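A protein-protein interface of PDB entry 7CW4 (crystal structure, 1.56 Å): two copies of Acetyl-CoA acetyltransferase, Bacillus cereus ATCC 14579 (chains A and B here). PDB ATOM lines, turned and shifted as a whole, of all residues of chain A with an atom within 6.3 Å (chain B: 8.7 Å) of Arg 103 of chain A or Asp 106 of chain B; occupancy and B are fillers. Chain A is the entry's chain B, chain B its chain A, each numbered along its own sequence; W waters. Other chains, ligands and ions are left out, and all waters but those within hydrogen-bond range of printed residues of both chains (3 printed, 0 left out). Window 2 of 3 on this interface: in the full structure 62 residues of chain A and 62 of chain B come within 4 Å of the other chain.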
ATOM      1  N   SER A   2       8.936  14.927 -25.653  1.00  0.00           N
ATOM      2  CA  SER A   2      10.112  15.798 -26.012  1.00  0.00           C
ATOM      3  C   SER A   2       9.872  16.527 -27.345  1.00  0.00           C
ATOM      4  O   SER A   2      10.623  17.502 -27.624  1.00  0.00           O
ATOM      5  CB  SER A   2      11.393  14.994 -26.051  1.00  0.00           C
ATOM      6  OG  SER A   2      12.421  15.728 -26.694  1.00  0.00           O
ATOM      7  N   LYS A   3       8.927  16.044 -28.167  1.00  0.00           N
ATOM      8  CA  LYS A   3       8.394  16.780 -29.347  1.00  0.00           C
ATOM      9  C   LYS A   3       6.871  16.714 -29.358  1.00  0.00           C
ATOM     10  O   LYS A   3       6.285  15.736 -28.910  1.00  0.00           O
ATOM     11  CB  LYS A   3       8.898  16.233 -30.686  1.00  0.00           C
ATOM     12  CG  LYS A   3      10.307  16.664 -31.036  1.00  0.00           C
ATOM     13  CD  LYS A   3      10.467  17.057 -32.474  1.00  0.00           C
ATOM     14  CE  LYS A   3      11.644  17.982 -32.673  1.00  0.00           C
ATOM     15  NZ  LYS A   3      12.908  17.233 -32.508  1.00  0.00           N
ATOM     16  N   THR A   4       6.262  17.713 -29.970  1.00  0.00           N
ATOM     17  CA  THR A   4       4.812  17.827 -30.091  1.00  0.00           C
ATOM     18  C   THR A   4       4.453  17.548 -31.553  1.00  0.00           C
ATOM     19  O   THR A   4       5.104  18.108 -32.437  1.00  0.00           O
ATOM     20  CB  THR A   4       4.334  19.237 -29.685  1.00  0.00           C
ATOM     21  OG1 THR A   4       4.844  19.448 -28.360  1.00  0.00           O
ATOM     22  CG2 THR A   4       2.840  19.356 -29.750  1.00  0.00           C
ATOM     23  N   THR A  96       2.499  27.634 -29.967  1.00  0.00           N
ATOM     24  CA  THR A  96       3.874  27.452 -29.468  1.00  0.00           C
ATOM     25  C   THR A  96       3.875  27.300 -27.938  1.00  0.00           C
ATOM     26  O   THR A  96       4.731  26.547 -27.403  1.00  0.00           O
ATOM     27  CB  THR A  96       4.828  28.518 -30.001  1.00  0.00           C
ATOM     28  OG1 THR A  96       4.506  29.813 -29.486  1.00  0.00           O
ATOM     29  CG2 THR A  96       4.856  28.545 -31.516  1.00  0.00           C
ATOM     30  N   ALA A  98       1.385  25.772 -26.252  1.00  0.00           N
ATOM     31  CA  ALA A  98       0.919  24.369 -26.158  1.00  0.00           C
ATOM     32  C   ALA A  98       2.127  23.440 -26.367  1.00  0.00           C
ATOM     33  O   ALA A  98       2.326  22.494 -25.572  1.00  0.00           O
ATOM     34  CB  ALA A  98      -0.221  24.116 -27.103  1.00  0.00           C
ATOM     35  N   ASP A  99       2.972  23.748 -27.342  1.00  0.00           N
ATOM     36  CA  ASP A  99       4.188  22.937 -27.611  1.00  0.00           C
ATOM     37  C   ASP A  99       5.081  22.893 -26.369  1.00  0.00           C
ATOM     38  O   ASP A  99       5.559  21.808 -25.975  1.00  0.00           O
ATOM     39  CB  ASP A  99       4.952  23.459 -28.835  1.00  0.00           C
ATOM     40  CG  ASP A  99       6.339  22.829 -29.009  1.00  0.00           C
ATOM     41  OD1 ASP A  99       6.384  21.643 -29.382  1.00  0.00           O
ATOM     42  OD2 ASP A  99       7.322  23.487 -28.697  1.00  0.00           O
ATOM     43  N   GLN A 100       5.323  24.053 -25.763  1.00  0.00           N
ATOM     44  CA  GLN A 100       6.199  24.128 -24.575  1.00  0.00           C
ATOM     45  C   GLN A 100       5.602  23.324 -23.415  1.00  0.00           C
ATOM     46  O   GLN A 100       6.327  22.567 -22.755  1.00  0.00           O
ATOM     47  CB  GLN A 100       6.422  25.605 -24.215  1.00  0.00           C
ATOM     48  CG  GLN A 100       7.230  26.304 -25.280  1.00  0.00           C
ATOM     49  CD  GLN A 100       7.404  27.779 -24.994  1.00  0.00           C
ATOM     50  OE1 GLN A 100       6.433  28.511 -24.829  1.00  0.00           O
ATOM     51  NE2 GLN A 100       8.635  28.227 -24.968  1.00  0.00           N
ATOM     52  N   ILE A 101       4.310  23.461 -23.152  1.00  0.00           N
ATOM     53  CA  ILE A 101       3.645  22.731 -22.027  1.00  0.00           C
ATOM     54  C   ILE A 101       3.743  21.228 -22.309  1.00  0.00           C
ATOM     55  O   ILE A 101       4.073  20.462 -21.381  1.00  0.00           O
ATOM     56  CB  ILE A 101       2.199  23.191 -21.866  1.00  0.00           C
ATOM     57  CG1 ILE A 101       2.188  24.646 -21.379  1.00  0.00           C
ATOM     58  CG2 ILE A 101       1.459  22.246 -20.948  1.00  0.00           C
ATOM     59  CD1 ILE A 101       0.848  25.292 -21.523  1.00  0.00           C
ATOM     60  N   ILE A 102       3.473  20.816 -23.528  1.00  0.00           N
ATOM     61  CA  ILE A 102       3.547  19.362 -23.866  1.00  0.00           C
ATOM     62  C   ILE A 102       4.971  18.867 -23.629  1.00  0.00           C
ATOM     63  O   ILE A 102       5.130  17.801 -23.012  1.00  0.00           O
ATOM     64  CB  ILE A 102       2.990  19.075 -25.262  1.00  0.00           C
ATOM     65  CG1 ILE A 102       1.465  19.171 -25.206  1.00  0.00           C
ATOM     66  CG2 ILE A 102       3.462  17.698 -25.786  1.00  0.00           C
ATOM     67  CD1 ILE A 102       0.776  19.283 -26.518  1.00  0.00           C
ATOM     68  N   ARG A 103       5.966  19.626 -24.031  1.00  0.00           N
ATOM     69  CA  ARG A 103       7.395  19.284 -23.895  1.00  0.00           C
ATOM     70  C   ARG A 103       7.795  19.134 -22.428  1.00  0.00           C
ATOM     71  O   ARG A 103       8.716  18.383 -22.181  1.00  0.00           O
ATOM     72  CB  ARG A 103       8.264  20.261 -24.675  1.00  0.00           C
ATOM     73  CG  ARG A 103       8.230  19.964 -26.172  1.00  0.00           C
ATOM     74  CD  ARG A 103       8.766  21.085 -27.005  1.00  0.00           C
ATOM     75  NE  ARG A 103      10.082  21.454 -26.552  1.00  0.00           N
ATOM     76  CZ  ARG A 103      10.497  22.673 -26.346  1.00  0.00           C
ATOM     77  NH1 ARG A 103      11.683  22.872 -25.828  1.00  0.00           N
ATOM     78  NH2 ARG A 103       9.767  23.722 -26.697  1.00  0.00           N
ATOM     79  N   THR A 104       7.110  19.757 -21.466  1.00  0.00           N
ATOM     80  CA  THR A 104       7.436  19.559 -20.035  1.00  0.00           C
ATOM     81  C   THR A 104       6.957  18.185 -19.574  1.00  0.00           C
ATOM     82  O   THR A 104       7.432  17.766 -18.509  1.00  0.00           O
ATOM     83  CB  THR A 104       6.797  20.604 -19.120  1.00  0.00           C
ATOM     84  OG1 THR A 104       5.398  20.370 -19.110  1.00  0.00           O
ATOM     85  CG2 THR A 104       7.185  22.018 -19.470  1.00  0.00           C
ATOM     86  N   GLY A 105       5.968  17.613 -20.239  1.00  0.00           N
ATOM     87  CA  GLY A 105       5.260  16.396 -19.818  1.00  0.00           C
ATOM     88  C   GLY A 105       4.083  16.714 -18.914  1.00  0.00           C
ATOM     89  O   GLY A 105       3.389  15.776 -18.534  1.00  0.00           O
ATOM     90  N   ASP A 106       3.810  17.994 -18.601  1.00  0.00           N
ATOM     91  CA  ASP A 106       2.675  18.329 -17.703  1.00  0.00           C
ATOM     92  C   ASP A 106       1.334  17.989 -18.340  1.00  0.00           C
ATOM     93  O   ASP A 106       0.418  17.601 -17.627  1.00  0.00           O
ATOM     94  CB  ASP A 106       2.702  19.799 -17.294  1.00  0.00           C
ATOM     95  CG  ASP A 106       3.849  20.188 -16.389  1.00  0.00           C
ATOM     96  OD1 ASP A 106       4.640  19.292 -15.949  1.00  0.00           O
ATOM     97  OD2 ASP A 106       3.963  21.388 -16.115  1.00  0.00           O
ATOM     98  N   GLN A 107       1.202  18.166 -19.655  1.00  0.00           N
ATOM     99  CA  GLN A 107       0.027  17.734 -20.429  1.00  0.00           C
ATOM    100  C   GLN A 107       0.501  16.980 -21.681  1.00  0.00           C
ATOM    101  O   GLN A 107       1.663  17.194 -22.071  1.00  0.00           O
ATOM    102  CB  GLN A 107      -0.815  18.945 -20.864  1.00  0.00           C
ATOM    103  CG  GLN A 107      -1.136  19.903 -19.706  1.00  0.00           C
ATOM    104  CD  GLN A 107      -2.002  19.288 -18.628  1.00  0.00           C
ATOM    105  OE1 GLN A 107      -2.624  18.262 -18.784  1.00  0.00           O
ATOM    106  NE2 GLN A 107      -1.994  19.884 -17.447  1.00  0.00           N
ATOM    107  N   HIS A 279      10.500  26.641 -32.566  1.00  0.00           N
ATOM    108  CA  HIS A 279       9.934  27.993 -32.768  1.00  0.00           C
ATOM    109  C   HIS A 279      10.822  28.992 -32.062  1.00  0.00           C
ATOM    110  O   HIS A 279      11.632  28.595 -31.148  1.00  0.00           O
ATOM    111  CB  HIS A 279       8.503  28.054 -32.253  1.00  0.00           C
ATOM    112  CG  HIS A 279       8.293  27.428 -30.931  1.00  0.00           C
ATOM    113  ND1 HIS A 279       8.518  28.129 -29.761  1.00  0.00           N
ATOM    114  CD2 HIS A 279       7.868  26.198 -30.582  1.00  0.00           C
ATOM    115  CE1 HIS A 279       8.266  27.312 -28.761  1.00  0.00           C
ATOM    116  NE2 HIS A 279       7.871  26.119 -29.221  1.00  0.00           N
ATOM    117  N   LYS A 303      18.861  28.947 -34.941  1.00  0.00           N
ATOM    118  CA  LYS A 303      18.602  28.081 -33.770  1.00  0.00           C
ATOM    119  C   LYS A 303      18.610  26.613 -34.191  1.00  0.00           C
ATOM    120  O   LYS A 303      19.035  25.754 -33.382  1.00  0.00           O
ATOM    121  CB  LYS A 303      17.280  28.520 -33.121  1.00  0.00           C
ATOM    122  CG  LYS A 303      16.722  27.545 -32.100  1.00  0.00           C
ATOM    123  CD  LYS A 303      15.430  28.050 -31.519  1.00  0.00           C
ATOM    124  CE  LYS A 303      14.825  27.064 -30.545  1.00  0.00           C
ATOM    125  NZ  LYS A 303      13.831  27.735 -29.687  1.00  0.00           N
ATOM    126  N   GLU B  49      14.217  37.645 -20.401  1.00  0.00           N
ATOM    127  CA  GLU B  49      14.038  36.963 -21.693  1.00  0.00           C
ATOM    128  C   GLU B  49      12.568  36.933 -22.112  1.00  0.00           C
ATOM    129  O   GLU B  49      12.321  36.824 -23.315  1.00  0.00           O
ATOM    130  CB  GLU B  49      14.567  35.552 -21.635  1.00  0.00           C
ATOM    131  CG  GLU B  49      16.067  35.549 -21.456  1.00  0.00           C
ATOM    132  CD  GLU B  49      16.629  34.155 -21.308  1.00  0.00           C
ATOM    133  OE1 GLU B  49      16.066  33.338 -20.604  1.00  0.00           O
ATOM    134  OE2 GLU B  49      17.657  33.885 -21.944  1.00  0.00           O
ATOM    135  N   GLU B  50      11.651  37.028 -21.154  1.00  0.00           N
ATOM    136  CA  GLU B  50      10.197  36.999 -21.465  1.00  0.00           C
ATOM    137  C   GLU B  50       9.455  37.651 -20.301  1.00  0.00           C
ATOM    138  O   GLU B  50       9.906  37.485 -19.148  1.00  0.00           O
ATOM    139  CB  GLU B  50       9.718  35.573 -21.702  1.00  0.00           C
ATOM    140  CG  GLU B  50       8.300  35.458 -22.242  1.00  0.00           C
ATOM    141  CD  GLU B  50       8.015  34.087 -22.856  1.00  0.00           C
ATOM    142  OE1 GLU B  50       8.962  33.257 -22.917  1.00  0.00           O
ATOM    143  OE2 GLU B  50       6.845  33.834 -23.284  1.00  0.00           O
ATOM    144  N   GLN B  80      10.584  39.712 -25.368  1.00  0.00           N
ATOM    145  CA  GLN B  80       9.293  39.185 -25.837  1.00  0.00           C
ATOM    146  C   GLN B  80       8.300  39.164 -24.661  1.00  0.00           C
ATOM    147  O   GLN B  80       8.724  39.082 -23.488  1.00  0.00           O
ATOM    148  CB  GLN B  80       9.439  37.826 -26.470  1.00  0.00           C
ATOM    149  CG  GLN B  80       9.887  36.769 -25.518  1.00  0.00           C
ATOM    150  CD  GLN B  80      10.098  35.493 -26.294  1.00  0.00           C
ATOM    151  OE1 GLN B  80       9.214  34.674 -26.362  1.00  0.00           O
ATOM    152  NE2 GLN B  80      11.315  35.271 -26.753  1.00  0.00           N
ATOM    153  N   ALA B  98       5.319  30.572 -16.753  1.00  0.00           N
ATOM    154  CA  ALA B  98       6.760  30.923 -16.705  1.00  0.00           C
ATOM    155  C   ALA B  98       7.538  29.703 -16.196  1.00  0.00           C
ATOM    156  O   ALA B  98       8.565  29.365 -16.768  1.00  0.00           O
ATOM    157  CB  ALA B  98       7.026  32.134 -15.839  1.00  0.00           C
ATOM    158  N   ASP B  99       7.038  29.035 -15.171  1.00  0.00           N
ATOM    159  CA  ASP B  99       7.691  27.807 -14.627  1.00  0.00           C
ATOM    160  C   ASP B  99       7.794  26.752 -15.751  1.00  0.00           C
ATOM    161  O   ASP B  99       8.841  26.051 -15.877  1.00  0.00           O
ATOM    162  CB  ASP B  99       6.892  27.217 -13.465  1.00  0.00           C
ATOM    163  CG  ASP B  99       7.402  25.836 -12.998  1.00  0.00           C
ATOM    164  OD1 ASP B  99       8.529  25.766 -12.417  1.00  0.00           O
ATOM    165  OD2 ASP B  99       6.695  24.867 -13.276  1.00  0.00           O
ATOM    166  N   GLN B 100       6.722  26.544 -16.492  1.00  0.00           N
ATOM    167  CA  GLN B 100       6.652  25.501 -17.551  1.00  0.00           C
ATOM    168  C   GLN B 100       7.664  25.867 -18.613  1.00  0.00           C
ATOM    169  O   GLN B 100       8.417  24.982 -19.096  1.00  0.00           O
ATOM    170  CB  GLN B 100       5.230  25.323 -18.095  1.00  0.00           C
ATOM    171  CG  GLN B 100       4.320  24.673 -17.055  1.00  0.00           C
ATOM    172  CD  GLN B 100       2.881  24.636 -17.477  1.00  0.00           C
ATOM    173  OE1 GLN B 100       2.294  25.610 -17.899  1.00  0.00           O
ATOM    174  NE2 GLN B 100       2.309  23.468 -17.401  1.00  0.00           N
ATOM    175  N   ILE B 101       7.678  27.119 -19.049  1.00  0.00           N
ATOM    176  CA  ILE B 101       8.631  27.520 -20.137  1.00  0.00           C
ATOM    177  C   ILE B 101      10.088  27.366 -19.662  1.00  0.00           C
ATOM    178  O   ILE B 101      10.927  26.834 -20.426  1.00  0.00           O
ATOM    179  CB  ILE B 101       8.338  28.940 -20.593  1.00  0.00           C
ATOM    180  CG1 ILE B 101       6.968  29.009 -21.284  1.00  0.00           C
ATOM    181  CG2 ILE B 101       9.480  29.465 -21.446  1.00  0.00           C
ATOM    182  CD1 ILE B 101       6.436  30.416 -21.397  1.00  0.00           C
ATOM    183  N   ILE B 102      10.404  27.781 -18.452  1.00  0.00           N
ATOM    184  CA  ILE B 102      11.782  27.597 -17.901  1.00  0.00           C
ATOM    185  C   ILE B 102      12.112  26.104 -17.829  1.00  0.00           C
ATOM    186  O   ILE B 102      13.241  25.740 -18.192  1.00  0.00           O
ATOM    187  CB  ILE B 102      11.959  28.376 -16.585  1.00  0.00           C
ATOM    188  CG1 ILE B 102      12.001  29.882 -16.855  1.00  0.00           C
ATOM    189  CG2 ILE B 102      13.194  27.876 -15.849  1.00  0.00           C
ATOM    190  CD1 ILE B 102      11.763  30.810 -15.669  1.00  0.00           C
ATOM    191  N   ARG B 103      11.166  25.245 -17.476  1.00  0.00           N
ATOM    192  CA  ARG B 103      11.433  23.802 -17.357  1.00  0.00           C
ATOM    193  C   ARG B 103      11.727  23.199 -18.725  1.00  0.00           C
ATOM    194  O   ARG B 103      12.401  22.163 -18.758  1.00  0.00           O
ATOM    195  CB  ARG B 103      10.310  23.089 -16.613  1.00  0.00           C
ATOM    196  CG  ARG B 103      10.428  23.353 -15.106  1.00  0.00           C
ATOM    197  CD  ARG B 103       9.156  23.063 -14.361  1.00  0.00           C
ATOM    198  NE  ARG B 103       8.715  21.751 -14.754  1.00  0.00           N
ATOM    199  CZ  ARG B 103       7.499  21.376 -15.044  1.00  0.00           C
ATOM    200  NH1 ARG B 103       7.285  20.133 -15.456  1.00  0.00           N
ATOM    201  NH2 ARG B 103       6.485  22.210 -14.985  1.00  0.00           N
ATOM    202  N   THR B 104      11.294  23.794 -19.830  1.00  0.00           N
ATOM    203  CA  THR B 104      11.650  23.272 -21.170  1.00  0.00           C
ATOM    204  C   THR B 104      13.125  23.562 -21.473  1.00  0.00           C
ATOM    205  O   THR B 104      13.641  22.925 -22.433  1.00  0.00           O
ATOM    206  CB  THR B 104      10.789  23.848 -22.302  1.00  0.00           C
ATOM    207  OG1 THR B 104      11.106  25.225 -22.460  1.00  0.00           O
ATOM    208  CG2 THR B 104       9.315  23.582 -22.111  1.00  0.00           C
ATOM    209  N   GLY B 105      13.750  24.539 -20.823  1.00  0.00           N
ATOM    210  CA  GLY B 105      15.037  25.103 -21.250  1.00  0.00           C
ATOM    211  C   GLY B 105      14.914  26.167 -22.317  1.00  0.00           C
ATOM    212  O   GLY B 105      15.936  26.765 -22.619  1.00  0.00           O
ATOM    213  N   ASP B 106      13.723  26.481 -22.840  1.00  0.00           N
ATOM    214  CA  ASP B 106      13.607  27.516 -23.908  1.00  0.00           C
ATOM    215  C   ASP B 106      14.028  28.893 -23.414  1.00  0.00           C
ATOM    216  O   ASP B 106      14.498  29.660 -24.210  1.00  0.00           O
ATOM    217  CB  ASP B 106      12.216  27.585 -24.538  1.00  0.00           C
ATOM    218  CG  ASP B 106      11.825  26.329 -25.300  1.00  0.00           C
ATOM    219  OD1 ASP B 106      12.672  25.403 -25.478  1.00  0.00           O
ATOM    220  OD2 ASP B 106      10.671  26.280 -25.758  1.00  0.00           O
ATOM    221  N   GLN B 107      13.756  29.220 -22.155  1.00  0.00           N
ATOM    222  CA  GLN B 107      14.151  30.488 -21.520  1.00  0.00           C
ATOM    223  C   GLN B 107      14.654  30.153 -20.115  1.00  0.00           C
ATOM    224  O   GLN B 107      14.311  29.092 -19.616  1.00  0.00           O
ATOM    225  CB  GLN B 107      12.967  31.467 -21.387  1.00  0.00           C
ATOM    226  CG  GLN B 107      12.232  31.763 -22.669  1.00  0.00           C
ATOM    227  CD  GLN B 107      13.092  32.393 -23.751  1.00  0.00           C
ATOM    228  OE1 GLN B 107      14.165  32.891 -23.543  1.00  0.00           O
ATOM    229  NE2 GLN B 107      12.650  32.281 -24.989  1.00  0.00           N
ATOM    230  N   SER B 108      15.473  31.004 -19.549  1.00  0.00           N
ATOM    231  CA  SER B 108      15.998  30.754 -18.190  1.00  0.00           C
ATOM    232  C   SER B 108      15.696  31.933 -17.240  1.00  0.00           C
ATOM    233  O   SER B 108      16.022  31.797 -16.057  1.00  0.00           O
ATOM    234  CB  SER B 108      17.486  30.427 -18.291  1.00  0.00           C
ATOM    235  OG  SER B 108      18.204  31.540 -18.798  1.00  0.00           O
ATOM    236  N   LEU B 109      15.117  33.049 -17.701  1.00  0.00           N
ATOM    237  CA  LEU B 109      14.856  34.249 -16.859  1.00  0.00           C
ATOM    238  C   LEU B 109      13.585  34.948 -17.362  1.00  0.00           C
ATOM    239  O   LEU B 109      13.554  35.556 -18.462  1.00  0.00           O
ATOM    240  CB  LEU B 109      16.079  35.178 -16.873  1.00  0.00           C
ATOM    241  CG  LEU B 109      15.985  36.504 -16.117  1.00  0.00           C
ATOM    242  CD1 LEU B 109      15.509  36.326 -14.698  1.00  0.00           C
ATOM    243  CD2 LEU B 109      17.329  37.242 -16.096  1.00  0.00           C
ATOM    244  N   ILE B 110      12.521  34.850 -16.560  1.00  0.00           N
ATOM    245  CA  ILE B 110      11.184  35.366 -16.969  1.00  0.00           C
ATOM    246  C   ILE B 110      10.664  36.226 -15.820  1.00  0.00           C
ATOM    247  O   ILE B 110      10.727  35.765 -14.636  1.00  0.00           O
ATOM    248  CB  ILE B 110      10.238  34.179 -17.264  1.00  0.00           C
ATOM    249  CG1 ILE B 110      10.790  33.317 -18.410  1.00  0.00           C
ATOM    250  CG2 ILE B 110       8.829  34.661 -17.581  1.00  0.00           C
ATOM    251  CD1 ILE B 110       9.891  32.181 -18.894  1.00  0.00           C
ATOM    252  N   SER B 261      15.783  29.647 -13.973  1.00  0.00           N
ATOM    253  CA  SER B 261      16.140  28.226 -13.812  1.00  0.00           C
ATOM    254  C   SER B 261      17.011  28.047 -12.553  1.00  0.00           C
ATOM    255  O   SER B 261      17.837  28.907 -12.278  1.00  0.00           O
ATOM    256  CB  SER B 261      16.842  27.651 -15.035  1.00  0.00           C
ATOM    257  OG  SER B 261      18.091  28.267 -15.206  1.00  0.00           O
HETATM  258  O   HOH W   1       9.179  31.129 -24.627  1.00  0.00           O
HETATM  259  O   HOH W   2      12.577  20.640 -23.622  1.00  0.00           O
HETATM  260  O   HOH W   3       9.552  18.723 -16.919  1.00  0.00           O
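OD2 of Asp 106 of chain A is in hydrogen-bond range of NE2 of Gln 100 of chain B.
The guanidinium group of Arg 103 of chain B is in salt-bridge range of the side-chain carboxylate of Asp 106 of chain A (2.8 Å).
The side-chain carboxylate (OD2) of Asp 106 of chain B sits at hydrogen-bond distance from the side-chain amide nitrogen (NE2) of Gln 100 of chain A (2.9 Å).
The side-chain carboxylate (OD1) of Asp 106 of chain B lies within salt-bridge range of the guanidinium group (NH1) of Arg 103 of chain A (2.7 Å).
The side-chain carboxylate (OD2) of Asp 99 of chain B is in salt-bridge range of the guanidinium group (NH2) of Arg 103 of chain B.
The backbone carbonyl oxygen of Ile 101 of chain B lies within hydrogen-bond range of the side-chain hydroxyl of Thr 104 of chain B.
The side-chain carboxylate (OD2) of Asp 99 of chain A is in salt-bridge range of the guanidinium group (NH2) of Arg 103 of chain A (3.2 Å).
The side-chain hydroxyl (OG1) of Thr 104 of chain A is in hydrogen-bond range of the backbone carbonyl oxygen (O) of Ile 101 of chain A, at 2.6 Å.
The backbone NH of Asp 106 of chain A lies within hydrogen-bond range of the side-chain hydroxyl of Thr 104 of chain A (2.9 Å).
The side-chain amino group of Lys 303 of chain A sits at hydrogen-bond distance from the backbone carbonyl oxygen of His 279 of chain A, at 2.8 Å.
Among the printed residues, pairs that only touch across the chains: Gln 100 of chain A with Thr 104 of chain B, Thr 104 of chain A with Gln 100 of chain B, Ile 101 of chain A with Gln 100 of chain B, Gln 100 of chain A with Ile 101 of chain B, Thr 104 of chain A with Arg 103 of chain B, Thr 104 of chain A with Thr 104 of chain B, Arg 103 of chain A with Thr 104 of chain B and His 279 of chain A with Asp 106 of chain B.
Printed residues of chain B within 4 Å of Gln 100 of chain A: Ile 101, Thr 104 and Asp 106.
Printed residues of chain B within 4 Å of Arg 103 of chain A: Thr 104 and Asp 106.
Thr 104 of chain A touches three residues of chain B.
Of the printed residues of chain B, Asp 106 of chain A touches Gln 100 (3.0 Å) and Arg 103 (2.8 Å).
Of the printed residues of chain A, Gln 100 of chain B touches Ile 101 (3.6 Å), Thr 104 (3.2 Å) and Asp 106 (3.0 Å).
Of the printed residues of chain A, Ile 101 of chain B touches Gln 100.
Printed residues of chain A within 4 Å of Arg 103 of chain B: Thr 104 (3.7 Å) and Asp 106 (2.8 Å).
Of the printed residues of chain A, Asp 106 of chain B touches Gln 100 (2.9 Å), Arg 103 (2.7 Å) and His 279 (3.98 Å).
The nearest residue of chain B that does not touch Arg 103 of chain A is Gly 105 of chain B (5.7 Å).
The nearest printed residue of chain A that does not touch Asp 106 of chain B is Lys 303 of chain A (4.9 Å).
Of the 17 printed residues of chain B, 5 touch a printed residue of chain A.
Printed residues of chain B that touch a printed residue of chain A: Gln 100, Ile 101, Arg 103, Thr 104 and Asp 106.
Hydrophobic or aromatic side chains of chain B within 4 Å of the printed part of chain A: Ile 101.
Of the 16 printed residues of chain A, 6 touch a printed residue of chain B.
Printed residues of chain A that touch a printed residue of chain B: Gln 100, Ile 101, Arg 103, Thr 104, Asp 106 and His 279.
Among the printed residues, 12 pairs touch across the chains.
Gln 100 of chain A touches Ile 101 of chain B, and with the chains exchanged Ile 101 of chain A touches Gln 100 of chain B.
Gln 100 of chain A touches Thr 104 of chain B, and with the chains exchanged Thr 104 of chain A touches Gln 100 of chain B.
Gln 100 of chain A touches Asp 106 of chain B, and with the chains exchanged Asp 106 of chain A touches Gln 100 of chain B.
Thr 104 of chain A touches its own counterpart, Thr 104 of chain B.
Of the 12 pairs that touch across the chains among the printed residues, 11 have their exchanged pair printed and touching as well.
Water W1 bridges OE1 of Glu 50 of chain B and NE2 of Gln 100 of chain A.
Water W2 lies within hydrogen-bond range of the backbone carbonyl oxygen of Thr 104 of chain B and the guanidinium group of Arg 103 of chain A.
Water W3 bridges O of Thr 104 of chain A (2.8 Å) and NH1 of Arg 103 of chain B (3.0 Å).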
